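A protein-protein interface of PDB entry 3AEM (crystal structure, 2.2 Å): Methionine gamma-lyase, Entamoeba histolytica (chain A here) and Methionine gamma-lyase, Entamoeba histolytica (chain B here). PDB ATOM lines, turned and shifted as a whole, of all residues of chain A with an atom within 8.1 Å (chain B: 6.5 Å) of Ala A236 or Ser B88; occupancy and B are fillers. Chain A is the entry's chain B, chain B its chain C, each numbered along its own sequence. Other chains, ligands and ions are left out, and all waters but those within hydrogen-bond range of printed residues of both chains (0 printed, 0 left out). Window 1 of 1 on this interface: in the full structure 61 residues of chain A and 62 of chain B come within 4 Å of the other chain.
The backbone carbonyl oxygen of Lys A234 sits at hydrogen-bond distance from the guanidinium group of Arg A55 (2.9 Å).
The side-chain hydroxyl (OG) of Ser A89 sits at hydrogen-bond distance from the backbone carbonyl oxygen (O) of Gly A85.
OD2 of Asp A235 is in salt-bridge range of NZ of Lys A234 (2.8 Å).
The side-chain hydroxyl of Ser B82 sits at hydrogen-bond distance from the backbone NH of Gly B85 (3.1 Å).
O of Met B84 lies within hydrogen-bond range of OG of Ser B88 (3.3 Å).
The backbone carbonyl oxygen (O) of Ser B88 lies within hydrogen-bond range of the side-chain hydroxyl (OG1) of Thr B91, 3.3 Å away.
The backbone carbonyl oxygen (O) of Asp A235 sits at hydrogen-bond distance from the side-chain hydroxyl (OG) of Ser B88, 3.1 Å away.
The side-chain carboxylate (OD1) of Asp A235 is in hydrogen-bond range of the indole nitrogen (NE1) of Trp B118 (3.0 Å).
O of Gly A237 sits at hydrogen-bond distance from OG of Ser B82, 2.7 Å away.
O of Gly A237 lies within hydrogen-bond range of OG of Ser B238 (2.6 Å).
Arg A233 touches none of the printed residues of chain B.
Printed residues of chain B within 4 Å of Leu A239: Ser B82.
Gly B83 touches none of the printed residues of chain A.
Of the printed residues of chain A, Met B84 touches Arg A55, Lys A234, Asp A235 and Ala A236.
Ser B88 touches just these residues of chain A: Asp A235 and Ala A236.
Of the printed residues of chain A, Trp B118 touches Leu A92, Phe A231, Tyr A232 and Asp A235.
Of the printed residues of chain A, Ser B238 touches Gly A237 and Ser A238.
The nearest residue of chain B that does not touch Ala A236 is Ser B238 (4.3 Å).
Among the printed residues, merely in contact across the chains: Arg A55 with Ser B82 (3.98 Å), Arg A55 with Met B84 (3.6 Å), Gly A85 with Ala B236 (3.2 Å), Ser A88 with Ala B236 (3.5 Å), Leu A92 with Trp B118 (3.7 Å), Phe A122 with Leu B92 (3.8 Å), Phe A231 with Trp B118 (3.4 Å), Tyr A232 with Trp B118 (3.6 Å), Lys A234 with Met B84 (3.5 Å), Asp A235 with Met B84 (3.5 Å), Asp A235 with Leu B114 (3.6 Å), Ala A236 with Met B84 (3.8 Å), Ala A236 with Gly B85 (3.2 Å), Ala A236 with Ser B88 (3.5 Å), Gly A237 with Gly B85 (3.95 Å), Ser A238 with Ser B238 (3.8 Å) and Leu A239 with Ser B82 (3.9 Å).
Of the 20 printed residues of chain B, 9 touch a printed residue of chain A.
Of the 18 printed residues of chain A, 13 touch a printed residue of chain B.
Hydrophobic or aromatic side chains of chain A that line the printed part of chain B: Phe A122, Phe A231, Tyr A232 and Leu A239.
Among the printed residues, 21 pairs touch across the chains.
Among the printed residues, no Asp or Glu carboxylate lies within 4 Å of a Lys or Arg side-chain nitrogen of the other chain.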
ATOM      1  N   ARG A  55      -3.060  12.275  -7.359  1.00  0.00           N
ATOM      2  CA  ARG A  55      -1.658  12.415  -6.971  1.00  0.00           C
ATOM      3  C   ARG A  55      -0.834  13.140  -8.062  1.00  0.00           C
ATOM      4  O   ARG A  55       0.096  13.869  -7.731  1.00  0.00           O
ATOM      5  CB  ARG A  55      -0.983  11.075  -6.589  1.00  0.00           C
ATOM      6  CG  ARG A  55       0.555  11.211  -6.176  1.00  0.00           C
ATOM      7  CD  ARG A  55       1.096  10.032  -5.266  1.00  0.00           C
ATOM      8  NE  ARG A  55       0.603   8.773  -5.783  1.00  0.00           N
ATOM      9  CZ  ARG A  55       1.004   8.200  -6.922  1.00  0.00           C
ATOM     10  NH1 ARG A  55       2.011   8.731  -7.632  1.00  0.00           N
ATOM     11  NH2 ARG A  55       0.440   7.059  -7.305  1.00  0.00           N
ATOM     12  N   PHE A  80       1.356  20.881  -1.103  1.00  0.00           N
ATOM     13  CA  PHE A  80       1.703  19.678  -0.356  1.00  0.00           C
ATOM     14  C   PHE A  80       0.796  19.558   0.880  1.00  0.00           C
ATOM     15  O   PHE A  80       0.080  20.498   1.254  1.00  0.00           O
ATOM     16  CB  PHE A  80       3.171  19.751   0.101  1.00  0.00           C
ATOM     17  CG  PHE A  80       4.153  19.906  -1.027  1.00  0.00           C
ATOM     18  CD1 PHE A  80       4.755  18.791  -1.603  1.00  0.00           C
ATOM     19  CD2 PHE A  80       4.473  21.172  -1.523  1.00  0.00           C
ATOM     20  CE1 PHE A  80       5.653  18.929  -2.659  1.00  0.00           C
ATOM     21  CE2 PHE A  80       5.362  21.310  -2.577  1.00  0.00           C
ATOM     22  CZ  PHE A  80       5.946  20.171  -3.145  1.00  0.00           C
ATOM     23  N   GLY A  85       6.395  18.951   4.033  1.00  0.00           N
ATOM     24  CA  GLY A  85       6.372  18.376   2.673  1.00  0.00           C
ATOM     25  C   GLY A  85       6.921  19.346   1.607  1.00  0.00           C
ATOM     26  O   GLY A  85       7.669  18.938   0.690  1.00  0.00           O
ATOM     27  N   SER A  88      10.875  19.452   2.364  1.00  0.00           N
ATOM     28  CA  SER A  88      11.485  18.193   1.944  1.00  0.00           C
ATOM     29  C   SER A  88      11.572  18.097   0.448  1.00  0.00           C
ATOM     30  O   SER A  88      12.615  17.746  -0.092  1.00  0.00           O
ATOM     31  CB  SER A  88      10.626  17.016   2.402  1.00  0.00           C
ATOM     32  OG  SER A  88      10.979  16.705   3.697  1.00  0.00           O
ATOM     33  N   SER A  89      10.465  18.388  -0.224  1.00  0.00           N
ATOM     34  CA  SER A  89      10.406  18.314  -1.683  1.00  0.00           C
ATOM     35  C   SER A  89      11.141  19.463  -2.390  1.00  0.00           C
ATOM     36  O   SER A  89      11.464  19.347  -3.558  1.00  0.00           O
ATOM     37  CB  SER A  89       8.950  18.271  -2.145  1.00  0.00           C
ATOM     38  OG  SER A  89       8.185  17.366  -1.346  1.00  0.00           O
ATOM     39  N   LEU A  92      15.272  17.875  -1.188  1.00  0.00           N
ATOM     40  CA  LEU A  92      15.658  16.513  -1.560  1.00  0.00           C
ATOM     41  C   LEU A  92      15.315  16.187  -2.994  1.00  0.00           C
ATOM     42  O   LEU A  92      15.765  15.170  -3.521  1.00  0.00           O
ATOM     43  CB  LEU A  92      14.988  15.485  -0.631  1.00  0.00           C
ATOM     44  CG  LEU A  92      15.518  15.473   0.808  1.00  0.00           C
ATOM     45  CD1 LEU A  92      14.676  14.628   1.775  1.00  0.00           C
ATOM     46  CD2 LEU A  92      16.999  15.037   0.842  1.00  0.00           C
ATOM     47  N   PHE A 122      21.286  10.597   4.045  1.00  0.00           N
ATOM     48  CA  PHE A 122      21.230  10.455   2.588  1.00  0.00           C
ATOM     49  C   PHE A 122      22.544  10.918   1.892  1.00  0.00           C
ATOM     50  O   PHE A 122      22.591  11.114   0.688  1.00  0.00           O
ATOM     51  CB  PHE A 122      19.967  11.122   2.024  1.00  0.00           C
ATOM     52  CG  PHE A 122      18.686  10.658   2.689  1.00  0.00           C
ATOM     53  CD1 PHE A 122      17.665  11.551   2.959  1.00  0.00           C
ATOM     54  CD2 PHE A 122      18.489   9.309   3.007  1.00  0.00           C
ATOM     55  CE1 PHE A 122      16.460  11.125   3.580  1.00  0.00           C
ATOM     56  CE2 PHE A 122      17.302   8.869   3.639  1.00  0.00           C
ATOM     57  CZ  PHE A 122      16.285   9.791   3.934  1.00  0.00           C
ATOM     58  N   ILE A 229      10.290  19.338  -8.781  1.00  0.00           N
ATOM     59  CA  ILE A 229       9.565  19.313  -7.506  1.00  0.00           C
ATOM     60  C   ILE A 229       8.324  18.402  -7.556  1.00  0.00           C
ATOM     61  O   ILE A 229       8.147  17.547  -6.687  1.00  0.00           O
ATOM     62  CB  ILE A 229       9.219  20.763  -7.001  1.00  0.00           C
ATOM     63  CG1 ILE A 229      10.500  21.481  -6.584  1.00  0.00           C
ATOM     64  CG2 ILE A 229       8.250  20.697  -5.826  1.00  0.00           C
ATOM     65  CD1 ILE A 229      10.413  23.001  -6.543  1.00  0.00           C
ATOM     66  N   LYS A 230       7.499  18.542  -8.595  1.00  0.00           N
ATOM     67  CA  LYS A 230       6.286  17.717  -8.733  1.00  0.00           C
ATOM     68  C   LYS A 230       6.602  16.238  -9.042  1.00  0.00           C
ATOM     69  O   LYS A 230       5.823  15.342  -8.695  1.00  0.00           O
ATOM     70  CB  LYS A 230       5.333  18.296  -9.779  1.00  0.00           C
ATOM     71  CG  LYS A 230       4.744  19.591  -9.353  1.00  0.00           C
ATOM     72  CD  LYS A 230       3.800  20.250 -10.384  1.00  0.00           C
ATOM     73  CE  LYS A 230       3.122  21.475  -9.722  1.00  0.00           C
ATOM     74  NZ  LYS A 230       2.285  22.363 -10.625  1.00  0.00           N
ATOM     75  N   PHE A 231       7.747  16.000  -9.666  1.00  0.00           N
ATOM     76  CA  PHE A 231       8.217  14.660  -9.911  1.00  0.00           C
ATOM     77  C   PHE A 231       8.605  14.001  -8.584  1.00  0.00           C
ATOM     78  O   PHE A 231       8.291  12.823  -8.337  1.00  0.00           O
ATOM     79  CB  PHE A 231       9.393  14.664 -10.904  1.00  0.00           C
ATOM     80  CG  PHE A 231       9.821  13.297 -11.295  1.00  0.00           C
ATOM     81  CD1 PHE A 231       9.071  12.548 -12.205  1.00  0.00           C
ATOM     82  CD2 PHE A 231      10.953  12.720 -10.725  1.00  0.00           C
ATOM     83  CE1 PHE A 231       9.456  11.232 -12.532  1.00  0.00           C
ATOM     84  CE2 PHE A 231      11.337  11.414 -11.039  1.00  0.00           C
ATOM     85  CZ  PHE A 231      10.589  10.672 -11.933  1.00  0.00           C
ATOM     86  N   TYR A 232       9.279  14.763  -7.723  1.00  0.00           N
ATOM     87  CA  TYR A 232       9.595  14.295  -6.395  1.00  0.00           C
ATOM     88  C   TYR A 232       8.324  14.072  -5.601  1.00  0.00           C
ATOM     89  O   TYR A 232       8.220  13.081  -4.910  1.00  0.00           O
ATOM     90  CB  TYR A 232      10.474  15.307  -5.664  1.00  0.00           C
ATOM     91  CG  TYR A 232      10.896  14.843  -4.288  1.00  0.00           C
ATOM     92  CD1 TYR A 232      10.101  15.105  -3.177  1.00  0.00           C
ATOM     93  CD2 TYR A 232      12.089  14.150  -4.101  1.00  0.00           C
ATOM     94  CE1 TYR A 232      10.469  14.686  -1.908  1.00  0.00           C
ATOM     95  CE2 TYR A 232      12.482  13.725  -2.825  1.00  0.00           C
ATOM     96  CZ  TYR A 232      11.658  14.004  -1.738  1.00  0.00           C
ATOM     97  OH  TYR A 232      12.015  13.621  -0.472  1.00  0.00           O
ATOM     98  N   ARG A 233       7.380  15.013  -5.682  1.00  0.00           N
ATOM     99  CA  ARG A 233       6.112  14.937  -4.946  1.00  0.00           C
ATOM    100  C   ARG A 233       5.320  13.660  -5.314  1.00  0.00           C
ATOM    101  O   ARG A 233       4.709  13.045  -4.437  1.00  0.00           O
ATOM    102  CB  ARG A 233       5.245  16.205  -5.159  1.00  0.00           C
ATOM    103  CG  ARG A 233       3.964  16.232  -4.296  1.00  0.00           C
ATOM    104  CD  ARG A 233       3.029  17.402  -4.576  1.00  0.00           C
ATOM    105  NE  ARG A 233       2.561  17.326  -5.960  1.00  0.00           N
ATOM    106  CZ  ARG A 233       1.861  18.256  -6.611  1.00  0.00           C
ATOM    107  NH1 ARG A 233       1.538  18.024  -7.876  1.00  0.00           N
ATOM    108  NH2 ARG A 233       1.441  19.378  -6.006  1.00  0.00           N
ATOM    109  N   LYS A 234       5.344  13.288  -6.599  1.00  0.00           N
ATOM    110  CA  LYS A 234       4.645  12.099  -7.122  1.00  0.00           C
ATOM    111  C   LYS A 234       5.121  10.779  -6.461  1.00  0.00           C
ATOM    112  O   LYS A 234       4.343   9.799  -6.330  1.00  0.00           O
ATOM    113  CB  LYS A 234       4.882  12.030  -8.645  1.00  0.00           C
ATOM    114  CG  LYS A 234       4.617  10.700  -9.334  1.00  0.00           C
ATOM    115  CD  LYS A 234       4.970  10.747 -10.837  1.00  0.00           C
ATOM    116  CE  LYS A 234       6.400  10.326 -11.099  1.00  0.00           C
ATOM    117  NZ  LYS A 234       6.631   8.890 -10.694  1.00  0.00           N
ATOM    118  N   ASP A 235       6.408  10.736  -6.117  1.00  0.00           N
ATOM    119  CA  ASP A 235       7.002   9.561  -5.468  1.00  0.00           C
ATOM    120  C   ASP A 235       7.056   9.686  -3.934  1.00  0.00           C
ATOM    121  O   ASP A 235       6.946   8.697  -3.224  1.00  0.00           O
ATOM    122  CB  ASP A 235       8.408   9.309  -6.044  1.00  0.00           C
ATOM    123  CG  ASP A 235       8.368   8.862  -7.498  1.00  0.00           C
ATOM    124  OD1 ASP A 235       9.429   8.927  -8.160  1.00  0.00           O
ATOM    125  OD2 ASP A 235       7.272   8.435  -7.974  1.00  0.00           O
ATOM    126  N   ALA A 236       7.242  10.901  -3.435  1.00  0.00           N
ATOM    127  CA  ALA A 236       7.318  11.138  -1.996  1.00  0.00           C
ATOM    128  C   ALA A 236       5.916  11.166  -1.367  1.00  0.00           C
ATOM    129  O   ALA A 236       5.742  10.767  -0.214  1.00  0.00           O
ATOM    130  CB  ALA A 236       8.035  12.449  -1.704  1.00  0.00           C
ATOM    131  N   GLY A 237       4.954  11.725  -2.094  1.00  0.00           N
ATOM    132  CA  GLY A 237       3.537  11.607  -1.721  1.00  0.00           C
ATOM    133  C   GLY A 237       2.946  12.508  -0.652  1.00  0.00           C
ATOM    134  O   GLY A 237       1.911  12.144  -0.031  1.00  0.00           O
ATOM    135  N   SER A 238       3.576  13.658  -0.420  1.00  0.00           N
ATOM    136  CA  SER A 238       2.948  14.703   0.405  1.00  0.00           C
ATOM    137  C   SER A 238       1.990  15.551  -0.453  1.00  0.00           C
ATOM    138  O   SER A 238       2.413  16.435  -1.187  1.00  0.00           O
ATOM    139  CB  SER A 238       3.986  15.563   1.121  1.00  0.00           C
ATOM    140  OG  SER A 238       3.347  16.565   1.910  1.00  0.00           O
ATOM    141  N   LEU A 239       0.694  15.221  -0.386  1.00  0.00           N
ATOM    142  CA  LEU A 239      -0.304  15.873  -1.236  1.00  0.00           C
ATOM    143  C   LEU A 239      -1.194  16.749  -0.389  1.00  0.00           C
ATOM    144  O   LEU A 239      -1.447  16.422   0.786  1.00  0.00           O
ATOM    145  CB  LEU A 239      -1.182  14.846  -1.956  1.00  0.00           C
ATOM    146  CG  LEU A 239      -0.381  13.740  -2.630  1.00  0.00           C
ATOM    147  CD1 LEU A 239      -1.379  12.748  -3.221  1.00  0.00           C
ATOM    148  CD2 LEU A 239       0.626  14.346  -3.696  1.00  0.00           C
ATOM    149  N   SER B  82      -0.831   9.672   0.846  1.00  0.00           N
ATOM    150  CA  SER B  82      -0.930   8.779  -0.338  1.00  0.00           C
ATOM    151  C   SER B  82      -0.264   7.457   0.008  1.00  0.00           C
ATOM    152  O   SER B  82       0.551   7.402   0.929  1.00  0.00           O
ATOM    153  CB  SER B  82      -0.212   9.404  -1.564  1.00  0.00           C
ATOM    154  OG  SER B  82       1.112   9.821  -1.232  1.00  0.00           O
ATOM    155  N   GLY B  83      -0.571   6.396  -0.741  1.00  0.00           N
ATOM    156  CA  GLY B  83       0.242   5.155  -0.681  1.00  0.00           C
ATOM    157  C   GLY B  83       1.734   5.430  -0.878  1.00  0.00           C
ATOM    158  O   GLY B  83       2.577   4.840  -0.195  1.00  0.00           O
ATOM    159  N   MET B  84       2.089   6.289  -1.835  1.00  0.00           N
ATOM    160  CA  MET B  84       3.491   6.630  -2.061  1.00  0.00           C
ATOM    161  C   MET B  84       4.121   7.242  -0.797  1.00  0.00           C
ATOM    162  O   MET B  84       5.320   7.022  -0.521  1.00  0.00           O
ATOM    163  CB  MET B  84       3.683   7.559  -3.287  1.00  0.00           C
ATOM    164  CG  MET B  84       3.408   6.869  -4.671  1.00  0.00           C
ATOM    165  SD  MET B  84       4.076   5.179  -4.793  1.00  0.00           S
ATOM    166  CE  MET B  84       5.846   5.413  -4.625  1.00  0.00           C
ATOM    167  N   GLY B  85       3.329   8.027  -0.056  1.00  0.00           N
ATOM    168  CA  GLY B  85       3.779   8.618   1.187  1.00  0.00           C
ATOM    169  C   GLY B  85       4.054   7.472   2.153  1.00  0.00           C
ATOM    170  O   GLY B  85       5.043   7.516   2.877  1.00  0.00           O
ATOM    171  N   ALA B  86       3.187   6.454   2.171  1.00  0.00           N
ATOM    172  CA  ALA B  86       3.400   5.343   3.095  1.00  0.00           C
ATOM    173  C   ALA B  86       4.663   4.583   2.712  1.00  0.00           C
ATOM    174  O   ALA B  86       5.429   4.166   3.591  1.00  0.00           O
ATOM    175  CB  ALA B  86       2.211   4.399   3.137  1.00  0.00           C
ATOM    176  N   ILE B  87       4.864   4.419   1.409  1.00  0.00           N
ATOM    177  CA  ILE B  87       5.982   3.634   0.896  1.00  0.00           C
ATOM    178  C   ILE B  87       7.322   4.329   1.139  1.00  0.00           C
ATOM    179  O   ILE B  87       8.229   3.693   1.628  1.00  0.00           O
ATOM    180  CB  ILE B  87       5.813   3.283  -0.586  1.00  0.00           C
ATOM    181  CG1 ILE B  87       4.677   2.256  -0.720  1.00  0.00           C
ATOM    182  CG2 ILE B  87       7.150   2.765  -1.149  1.00  0.00           C
ATOM    183  CD1 ILE B  87       4.146   2.039  -2.141  1.00  0.00           C
ATOM    184  N   SER B  88       7.444   5.609   0.770  1.00  0.00           N
ATOM    185  CA  SER B  88       8.607   6.440   1.117  1.00  0.00           C
ATOM    186  C   SER B  88       8.971   6.402   2.595  1.00  0.00           C
ATOM    187  O   SER B  88      10.133   6.289   2.971  1.00  0.00           O
ATOM    188  CB  SER B  88       8.312   7.920   0.802  1.00  0.00           C
ATOM    189  OG  SER B  88       8.464   8.116  -0.564  1.00  0.00           O
ATOM    190  N   SER B  89       7.954   6.563   3.425  1.00  0.00           N
ATOM    191  CA  SER B  89       8.167   6.657   4.871  1.00  0.00           C
ATOM    192  C   SER B  89       8.459   5.285   5.468  1.00  0.00           C
ATOM    193  O   SER B  89       8.980   5.202   6.567  1.00  0.00           O
ATOM    194  CB  SER B  89       6.958   7.306   5.578  1.00  0.00           C
ATOM    195  OG  SER B  89       6.591   8.559   4.990  1.00  0.00           O
ATOM    196  N   SER B  90       8.111   4.210   4.779  1.00  0.00           N
ATOM    197  CA  SER B  90       8.354   2.869   5.320  1.00  0.00           C
ATOM    198  C   SER B  90       9.715   2.354   4.848  1.00  0.00           C
ATOM    199  O   SER B  90      10.171   1.322   5.290  1.00  0.00           O
ATOM    200  CB  SER B  90       7.241   1.898   4.887  1.00  0.00           C
ATOM    201  OG  SER B  90       6.012   2.295   5.479  1.00  0.00           O
ATOM    202  N   THR B  91      10.341   3.055   3.914  1.00  0.00           N
ATOM    203  CA  THR B  91      11.635   2.627   3.443  1.00  0.00           C
ATOM    204  C   THR B  91      12.709   3.639   3.852  1.00  0.00           C
ATOM    205  O   THR B  91      13.679   3.256   4.513  1.00  0.00           O
ATOM    206  CB  THR B  91      11.603   2.413   1.926  1.00  0.00           C
ATOM    207  OG1 THR B  91      11.108   3.601   1.296  1.00  0.00           O
ATOM    208  CG2 THR B  91      10.636   1.263   1.581  1.00  0.00           C
ATOM    209  N   LEU B  92      12.543   4.914   3.494  1.00  0.00           N
ATOM    210  CA  LEU B  92      13.564   5.921   3.793  1.00  0.00           C
ATOM    211  C   LEU B  92      13.669   6.284   5.289  1.00  0.00           C
ATOM    212  O   LEU B  92      14.662   6.873   5.742  1.00  0.00           O
ATOM    213  CB  LEU B  92      13.310   7.174   2.942  1.00  0.00           C
ATOM    214  CG  LEU B  92      13.417   6.947   1.430  1.00  0.00           C
ATOM    215  CD1 LEU B  92      13.018   8.220   0.687  1.00  0.00           C
ATOM    216  CD2 LEU B  92      14.842   6.572   1.086  1.00  0.00           C
ATOM    217  N   ALA B  93      12.657   5.931   6.070  1.00  0.00           N
ATOM    218  CA  ALA B  93      12.775   6.060   7.531  1.00  0.00           C
ATOM    219  C   ALA B  93      13.855   5.140   8.101  1.00  0.00           C
ATOM    220  O   ALA B  93      14.424   5.447   9.155  1.00  0.00           O
ATOM    221  CB  ALA B  93      11.434   5.840   8.240  1.00  0.00           C
ATOM    222  N   PHE B  94      14.175   4.057   7.394  1.00  0.00           N
ATOM    223  CA  PHE B  94      15.176   3.083   7.883  1.00  0.00           C
ATOM    224  C   PHE B  94      16.467   2.988   7.047  1.00  0.00           C
ATOM    225  O   PHE B  94      17.546   2.804   7.591  1.00  0.00           O
ATOM    226  CB  PHE B  94      14.538   1.708   7.950  1.00  0.00           C
ATOM    227  CG  PHE B  94      13.293   1.687   8.787  1.00  0.00           C
ATOM    228  CD1 PHE B  94      12.050   1.713   8.184  1.00  0.00           C
ATOM    229  CD2 PHE B  94      13.381   1.686  10.168  1.00  0.00           C
ATOM    230  CE1 PHE B  94      10.916   1.720   8.959  1.00  0.00           C
ATOM    231  CE2 PHE B  94      12.269   1.672  10.930  1.00  0.00           C
ATOM    232  CZ  PHE B  94      11.012   1.700  10.325  1.00  0.00           C
ATOM    233  N   LEU B 114      10.453   5.542  -7.374  1.00  0.00           N
ATOM    234  CA  LEU B 114      11.084   5.827  -6.066  1.00  0.00           C
ATOM    235  C   LEU B 114      12.406   5.084  -5.866  1.00  0.00           C
ATOM    236  O   LEU B 114      13.433   5.706  -5.546  1.00  0.00           O
ATOM    237  CB  LEU B 114      10.125   5.486  -4.900  1.00  0.00           C
ATOM    238  CG  LEU B 114      10.608   5.743  -3.463  1.00  0.00           C
ATOM    239  CD1 LEU B 114      10.810   7.270  -3.174  1.00  0.00           C
ATOM    240  CD2 LEU B 114       9.578   5.147  -2.491  1.00  0.00           C
ATOM    241  N   PHE B 115      12.367   3.761  -6.081  1.00  0.00           N
ATOM    242  CA  PHE B 115      13.479   2.869  -5.775  1.00  0.00           C
ATOM    243  C   PHE B 115      14.609   3.016  -6.799  1.00  0.00           C
ATOM    244  O   PHE B 115      15.778   2.865  -6.459  1.00  0.00           O
ATOM    245  CB  PHE B 115      13.019   1.411  -5.763  1.00  0.00           C
ATOM    246  CG  PHE B 115      12.142   1.031  -4.577  1.00  0.00           C
ATOM    247  CD1 PHE B 115      11.561  -0.248  -4.523  1.00  0.00           C
ATOM    248  CD2 PHE B 115      11.892   1.929  -3.535  1.00  0.00           C
ATOM    249  CE1 PHE B 115      10.762  -0.654  -3.423  1.00  0.00           C
ATOM    250  CE2 PHE B 115      11.082   1.565  -2.459  1.00  0.00           C
ATOM    251  CZ  PHE B 115      10.514   0.253  -2.389  1.00  0.00           C
ATOM    252  N   TRP B 118      15.131   7.766  -6.898  1.00  0.00           N
ATOM    253  CA  TRP B 118      15.418   8.558  -5.707  1.00  0.00           C
ATOM    254  C   TRP B 118      16.367   7.854  -4.753  1.00  0.00           C
ATOM    255  O   TRP B 118      17.363   8.446  -4.399  1.00  0.00           O
ATOM    256  CB  TRP B 118      14.129   9.071  -5.029  1.00  0.00           C
ATOM    257  CG  TRP B 118      13.340   9.962  -5.927  1.00  0.00           C
ATOM    258  CD1 TRP B 118      12.161   9.652  -6.563  1.00  0.00           C
ATOM    259  CD2 TRP B 118      13.681  11.299  -6.345  1.00  0.00           C
ATOM    260  NE1 TRP B 118      11.737  10.717  -7.312  1.00  0.00           N
ATOM    261  CE2 TRP B 118      12.642  11.740  -7.204  1.00  0.00           C
ATOM    262  CE3 TRP B 118      14.740  12.178  -6.046  1.00  0.00           C
ATOM    263  CZ2 TRP B 118      12.639  13.015  -7.795  1.00  0.00           C
ATOM    264  CZ3 TRP B 118      14.739  13.446  -6.627  1.00  0.00           C
ATOM    265  CH2 TRP B 118      13.689  13.852  -7.491  1.00  0.00           C
ATOM    266  N   LEU B 200       1.854  -2.333   4.515  1.00  0.00           N
ATOM    267  CA  LEU B 200       1.367  -1.022   4.101  1.00  0.00           C
ATOM    268  C   LEU B 200       0.356  -1.146   2.975  1.00  0.00           C
ATOM    269  O   LEU B 200       0.277  -2.190   2.309  1.00  0.00           O
ATOM    270  CB  LEU B 200       2.527  -0.101   3.688  1.00  0.00           C
ATOM    271  CG  LEU B 200       3.404  -0.457   2.485  1.00  0.00           C
ATOM    272  CD1 LEU B 200       2.722   0.035   1.208  1.00  0.00           C
ATOM    273  CD2 LEU B 200       4.762   0.154   2.645  1.00  0.00           C
ATOM    274  N   TYR B 232       9.806  10.050  10.910  1.00  0.00           N
ATOM    275  CA  TYR B 232      10.064  10.375   9.514  1.00  0.00           C
ATOM    276  C   TYR B 232       8.920  11.245   8.925  1.00  0.00           C
ATOM    277  O   TYR B 232       9.177  12.310   8.319  1.00  0.00           O
ATOM    278  CB  TYR B 232      10.272   9.105   8.675  1.00  0.00           C
ATOM    279  CG  TYR B 232      10.618   9.403   7.219  1.00  0.00           C
ATOM    280  CD1 TYR B 232      11.938   9.623   6.829  1.00  0.00           C
ATOM    281  CD2 TYR B 232       9.619   9.483   6.247  1.00  0.00           C
ATOM    282  CE1 TYR B 232      12.267   9.928   5.507  1.00  0.00           C
ATOM    283  CE2 TYR B 232       9.921   9.750   4.912  1.00  0.00           C
ATOM    284  CZ  TYR B 232      11.247   9.984   4.544  1.00  0.00           C
ATOM    285  OH  TYR B 232      11.562  10.263   3.230  1.00  0.00           O
ATOM    286  N   ALA B 236       9.038  14.611   6.826  1.00  0.00           N
ATOM    287  CA  ALA B 236       8.783  14.499   5.364  1.00  0.00           C
ATOM    288  C   ALA B 236       7.389  15.065   4.979  1.00  0.00           C
ATOM    289  O   ALA B 236       7.177  15.523   3.840  1.00  0.00           O
ATOM    290  CB  ALA B 236       8.930  13.071   4.904  1.00  0.00           C
ATOM    291  N   SER B 238       4.117  13.944   4.681  1.00  0.00           N
ATOM    292  CA  SER B 238       2.977  13.297   4.005  1.00  0.00           C
ATOM    293  C   SER B 238       1.867  12.920   4.985  1.00  0.00           C
ATOM    294  O   SER B 238       1.926  11.900   5.660  1.00  0.00           O
ATOM    295  CB  SER B 238       3.392  12.097   3.154  1.00  0.00           C
ATOM    296  OG  SER B 238       2.220  11.579   2.506  1.00  0.00           O
